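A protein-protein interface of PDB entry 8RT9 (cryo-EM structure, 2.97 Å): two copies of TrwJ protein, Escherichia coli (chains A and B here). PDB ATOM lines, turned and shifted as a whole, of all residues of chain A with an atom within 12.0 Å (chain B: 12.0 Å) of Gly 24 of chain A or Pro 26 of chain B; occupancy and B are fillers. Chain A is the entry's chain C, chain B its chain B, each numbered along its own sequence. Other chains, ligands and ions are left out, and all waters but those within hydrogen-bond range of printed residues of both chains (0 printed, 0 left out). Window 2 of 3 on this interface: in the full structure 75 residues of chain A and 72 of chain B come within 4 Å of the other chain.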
ATOM      1  N   GLN A  23      -4.925 -16.711 -11.529  1.00  0.00           N
ATOM      2  CA  GLN A  23      -6.250 -16.628 -10.925  1.00  0.00           C
ATOM      3  C   GLN A  23      -6.480 -15.263 -10.295  1.00  0.00           C
ATOM      4  O   GLN A  23      -6.454 -14.243 -10.980  1.00  0.00           O
ATOM      5  CB  GLN A  23      -6.438 -17.726  -9.880  1.00  0.00           C
ATOM      6  N   GLY A  24      -6.698 -15.246  -8.986  1.00  0.00           N
ATOM      7  CA  GLY A  24      -7.087 -14.022  -8.318  1.00  0.00           C
ATOM      8  C   GLY A  24      -6.306 -13.780  -7.046  1.00  0.00           C
ATOM      9  O   GLY A  24      -6.066 -14.689  -6.252  1.00  0.00           O
ATOM     10  N   ILE A  25      -5.920 -12.522  -6.855  1.00  0.00           N
ATOM     11  CA  ILE A  25      -5.224 -12.080  -5.646  1.00  0.00           C
ATOM     12  C   ILE A  25      -3.998 -12.952  -5.421  1.00  0.00           C
ATOM     13  O   ILE A  25      -4.001 -13.791  -4.507  1.00  0.00           O
ATOM     14  CB  ILE A  25      -6.160 -12.120  -4.428  1.00  0.00           C
ATOM     15  N   PRO A  26      -2.946 -12.809  -6.219  1.00  0.00           N
ATOM     16  CA  PRO A  26      -1.777 -13.676  -6.055  1.00  0.00           C
ATOM     17  C   PRO A  26      -1.169 -13.530  -4.671  1.00  0.00           C
ATOM     18  O   PRO A  26      -1.125 -12.437  -4.104  1.00  0.00           O
ATOM     19  CB  PRO A  26      -0.814 -13.196  -7.147  1.00  0.00           C
ATOM     20  CG  PRO A  26      -1.613 -12.330  -8.050  1.00  0.00           C
ATOM     21  CD  PRO A  26      -2.773 -11.813  -7.283  1.00  0.00           C
ATOM     22  N   VAL A  27      -0.699 -14.650  -4.129  1.00  0.00           N
ATOM     23  CA  VAL A  27      -0.110 -14.706  -2.799  1.00  0.00           C
ATOM     24  C   VAL A  27       1.221 -15.436  -2.868  1.00  0.00           C
ATOM     25  O   VAL A  27       1.380 -16.407  -3.611  1.00  0.00           O
ATOM     26  CB  VAL A  27      -1.050 -15.380  -1.782  1.00  0.00           C
ATOM     27  CG1 VAL A  27      -0.332 -15.611  -0.484  1.00  0.00           C
ATOM     28  CG2 VAL A  27      -2.262 -14.496  -1.534  1.00  0.00           C
ATOM     29  N   PHE A  28       2.186 -14.944  -2.097  1.00  0.00           N
ATOM     30  CA  PHE A  28       3.514 -15.534  -2.004  1.00  0.00           C
ATOM     31  C   PHE A  28       3.648 -16.209  -0.651  1.00  0.00           C
ATOM     32  O   PHE A  28       3.835 -15.530   0.363  1.00  0.00           O
ATOM     33  CB  PHE A  28       4.589 -14.464  -2.174  1.00  0.00           C
ATOM     34  CG  PHE A  28       5.991 -14.991  -2.142  1.00  0.00           C
ATOM     35  CD1 PHE A  28       6.596 -15.439  -3.299  1.00  0.00           C
ATOM     36  CD2 PHE A  28       6.712 -15.011  -0.964  1.00  0.00           C
ATOM     37  CE1 PHE A  28       7.892 -15.918  -3.280  1.00  0.00           C
ATOM     38  CE2 PHE A  28       8.007 -15.485  -0.939  1.00  0.00           C
ATOM     39  CZ  PHE A  28       8.598 -15.940  -2.098  1.00  0.00           C
ATOM     40  N   ASP A  29       3.565 -17.535  -0.634  1.00  0.00           N
ATOM     41  CA  ASP A  29       3.730 -18.290   0.603  1.00  0.00           C
ATOM     42  C   ASP A  29       5.216 -18.393   0.905  1.00  0.00           C
ATOM     43  O   ASP A  29       5.874 -19.356   0.500  1.00  0.00           O
ATOM     44  CB  ASP A  29       3.107 -19.675   0.494  1.00  0.00           C
ATOM     45  CG  ASP A  29       1.594 -19.624   0.472  1.00  0.00           C
ATOM     46  OD1 ASP A  29       1.026 -18.570   0.822  1.00  0.00           O
ATOM     47  OD2 ASP A  29       0.961 -20.645   0.149  1.00  0.00           O
ATOM     48  N   GLN B  23     -13.290 -23.646  -3.112  1.00  0.00           N
ATOM     49  CA  GLN B  23     -13.529 -23.069  -1.795  1.00  0.00           C
ATOM     50  C   GLN B  23     -13.830 -21.583  -1.895  1.00  0.00           C
ATOM     51  O   GLN B  23     -14.808 -21.182  -2.522  1.00  0.00           O
ATOM     52  CB  GLN B  23     -12.328 -23.300  -0.878  1.00  0.00           C
ATOM     53  N   GLY B  24     -12.985 -20.765  -1.280  1.00  0.00           N
ATOM     54  CA  GLY B  24     -13.269 -19.350  -1.178  1.00  0.00           C
ATOM     55  C   GLY B  24     -12.075 -18.489  -1.527  1.00  0.00           C
ATOM     56  O   GLY B  24     -10.942 -18.768  -1.134  1.00  0.00           O
ATOM     57  N   ILE B  25     -12.351 -17.419  -2.266  1.00  0.00           N
ATOM     58  CA  ILE B  25     -11.340 -16.429  -2.635  1.00  0.00           C
ATOM     59  C   ILE B  25     -10.164 -17.129  -3.301  1.00  0.00           C
ATOM     60  O   ILE B  25      -9.094 -17.253  -2.685  1.00  0.00           O
ATOM     61  CB  ILE B  25     -10.879 -15.628  -1.406  1.00  0.00           C
ATOM     62  N   PRO B  26     -10.308 -17.611  -4.529  1.00  0.00           N
ATOM     63  CA  PRO B  26      -9.208 -18.337  -5.168  1.00  0.00           C
ATOM     64  C   PRO B  26      -7.969 -17.466  -5.294  1.00  0.00           C
ATOM     65  O   PRO B  26      -8.055 -16.265  -5.551  1.00  0.00           O
ATOM     66  CB  PRO B  26      -9.772 -18.715  -6.542  1.00  0.00           C
ATOM     67  CG  PRO B  26     -11.236 -18.472  -6.468  1.00  0.00           C
ATOM     68  CD  PRO B  26     -11.482 -17.471  -5.401  1.00  0.00           C
ATOM     69  N   VAL B  27      -6.809 -18.089  -5.105  1.00  0.00           N
ATOM     70  CA  VAL B  27      -5.522 -17.410  -5.156  1.00  0.00           C
ATOM     71  C   VAL B  27      -4.580 -18.184  -6.063  1.00  0.00           C
ATOM     72  O   VAL B  27      -4.584 -19.417  -6.085  1.00  0.00           O
ATOM     73  CB  VAL B  27      -4.909 -17.233  -3.755  1.00  0.00           C
ATOM     74  CG1 VAL B  27      -3.501 -16.727  -3.864  1.00  0.00           C
ATOM     75  CG2 VAL B  27      -5.737 -16.243  -2.951  1.00  0.00           C
ATOM     76  N   PHE B  28      -3.783 -17.445  -6.829  1.00  0.00           N
ATOM     77  CA  PHE B  28      -2.791 -18.012  -7.731  1.00  0.00           C
ATOM     78  C   PHE B  28      -1.412 -17.759  -7.151  1.00  0.00           C
ATOM     79  O   PHE B  28      -0.903 -16.637  -7.230  1.00  0.00           O
ATOM     80  CB  PHE B  28      -2.907 -17.385  -9.119  1.00  0.00           C
ATOM     81  CG  PHE B  28      -1.954 -17.947 -10.128  1.00  0.00           C
ATOM     82  CD1 PHE B  28      -2.295 -19.060 -10.869  1.00  0.00           C
ATOM     83  CD2 PHE B  28      -0.732 -17.344 -10.358  1.00  0.00           C
ATOM     84  CE1 PHE B  28      -1.426 -19.578 -11.808  1.00  0.00           C
ATOM     85  CE2 PHE B  28       0.139 -17.854 -11.298  1.00  0.00           C
ATOM     86  CZ  PHE B  28      -0.207 -18.974 -12.023  1.00  0.00           C
ATOM     87  N   ASP B  29      -0.804 -18.794  -6.580  1.00  0.00           N
ATOM     88  CA  ASP B  29       0.543 -18.677  -6.035  1.00  0.00           C
ATOM     89  C   ASP B  29       1.532 -18.751  -7.187  1.00  0.00           C
ATOM     90  O   ASP B  29       2.014 -19.832  -7.531  1.00  0.00           O
ATOM     91  CB  ASP B  29       0.824 -19.772  -5.014  1.00  0.00           C
ATOM     92  CG  ASP B  29       0.052 -19.570  -3.727  1.00  0.00           C
ATOM     93  OD1 ASP B  29      -0.470 -18.457  -3.514  1.00  0.00           O
ATOM     94  OD2 ASP B  29      -0.005 -20.501  -2.905  1.00  0.00           O
ATOM     95  N   GLY B  30       1.833 -17.602  -7.783  1.00  0.00           N
ATOM     96  CA  GLY B  30       2.642 -17.589  -8.989  1.00  0.00           C
ATOM     97  C   GLY B  30       3.998 -18.235  -8.807  1.00  0.00           C
ATOM     98  O   GLY B  30       4.569 -18.773  -9.757  1.00  0.00           O
ATOM     99  N   THR B  31       4.535 -18.187  -7.592  1.00  0.00           N
ATOM    100  CA  THR B  31       5.849 -18.765  -7.358  1.00  0.00           C
ATOM    101  C   THR B  31       5.825 -20.283  -7.451  1.00  0.00           C
ATOM    102  O   THR B  31       6.750 -20.880  -8.011  1.00  0.00           O
ATOM    103  CB  THR B  31       6.380 -18.324  -6.000  1.00  0.00           C
ATOM    104  OG1 THR B  31       6.494 -16.898  -5.987  1.00  0.00           O
ATOM    105  CG2 THR B  31       7.746 -18.932  -5.739  1.00  0.00           C
ATOM    106  N   ARG B  32       4.778 -20.925  -6.932  1.00  0.00           N
ATOM    107  CA  ARG B  32       4.761 -22.379  -6.923  1.00  0.00           C
ATOM    108  C   ARG B  32       4.711 -22.940  -8.335  1.00  0.00           C
ATOM    109  O   ARG B  32       5.171 -24.061  -8.574  1.00  0.00           O
ATOM    110  CB  ARG B  32       3.577 -22.894  -6.111  1.00  0.00           C
ATOM    111  CG  ARG B  32       3.531 -24.396  -5.994  1.00  0.00           C
ATOM    112  CD  ARG B  32       2.355 -24.883  -5.190  1.00  0.00           C
ATOM    113  NE  ARG B  32       1.082 -24.585  -5.827  1.00  0.00           N
ATOM    114  CZ  ARG B  32       0.263 -23.624  -5.421  1.00  0.00           C
ATOM    115  NH1 ARG B  32       0.587 -22.877  -4.373  1.00  0.00           N
ATOM    116  NH2 ARG B  32      -0.880 -23.410  -6.056  1.00  0.00           N
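The backbone carbonyl oxygen (O) of Gly 24 of chain A sits close to the backbone carbonyl oxygen (O) of Pro 26 of chain B (2.6 Å). OD1 of Asp 29 of chain B sits close to O of Val 27 of chain A (2.8 Å). The side-chain carboxylate (OD2) of Asp 29 of chain A sits close to the side-chain carboxylate (OD2) of Asp 29 of chain B (3.2 Å).
The side-chain carboxylate (OD2) of Asp 29 of chain B lies within salt-bridge range of the guanidinium group (NH1) of Arg 32 of chain B (2.9 Å).
Among the printed residues, pairs that only touch across the chains: Gln 23 of chain A with Phe 28 of chain B, Gly 24 of chain A with Val 27 of chain B, Gly 24 of chain A with Phe 28 of chain B, Ile 25 of chain A with Val 27 of chain B, Pro 26 of chain A with Phe 28 of chain B, Val 27 of chain A with Val 27 of chain B, Val 27 of chain A with Phe 28 of chain B and Phe 28 of chain A with Thr 31 of chain B.
Gly 24 of chain A touches just these residues of chain B: Pro 26 (2.6 Å), Val 27 (3.0 Å) and Phe 28 (3.6 Å). Pro 26 of chain B touches one residue of chain A. Of chain B, only Phe 28 (3.2 Å) comes within 4 Å of Gln 23 of chain A. Ile 25 of chain A touches just one residue of chain B: Val 27. Pro 26 of chain A touches just one residue of chain B: Phe 28. No residue of chain A comes within 4 Å of Gln 23 of chain B. Val 27 of chain B touches three residues of chain A. Of the printed residues of chain B, Phe 28 of chain A touches Thr 31 (3.1 Å). Of the printed residues of chain A, Thr 31 of chain B touches Phe 28. Of the printed residues of chain B, Val 27 of chain A touches Val 27 (3.5 Å), Phe 28 (3.7 Å) and Asp 29 (2.8 Å). Printed residues of chain B within 4 Å of Asp 29 of chain A: Asp 29 (3.2 Å). Of the printed residues of chain A, Phe 28 of chain B touches Gln 23, Gly 24, Pro 26 and Val 27. The nearest residue of chain B that does not touch Gly 24 of chain A is Ile 25 of chain B (5.3 Å). The nearest residue of chain A that does not touch Pro 26 of chain B is Ile 25 of chain A (4.5 Å). The nearest printed residue of chain B that does not touch Val 27 of chain A is Gly 30 of chain B (4.4 Å).
Among the printed residues, 11 pairs touch across the chains.
Gly 24 of chain A touches Pro 26 of chain B, but with the chains exchanged Pro 26 of chain A does not touch Gly 24 of chain B (11.2 Å). Gly 24 of chain A touches Phe 28 of chain B, but with the chains exchanged Phe 28 of chain A does not touch Gly 24 of chain B (13.7 Å). Val 27 of chain A touches Phe 28 of chain B, but with the chains exchanged Phe 28 of chain A does not touch Val 27 of chain B (6.2 Å). Asp 29 of chain B touches its own counterpart, Asp 29 of chain A.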
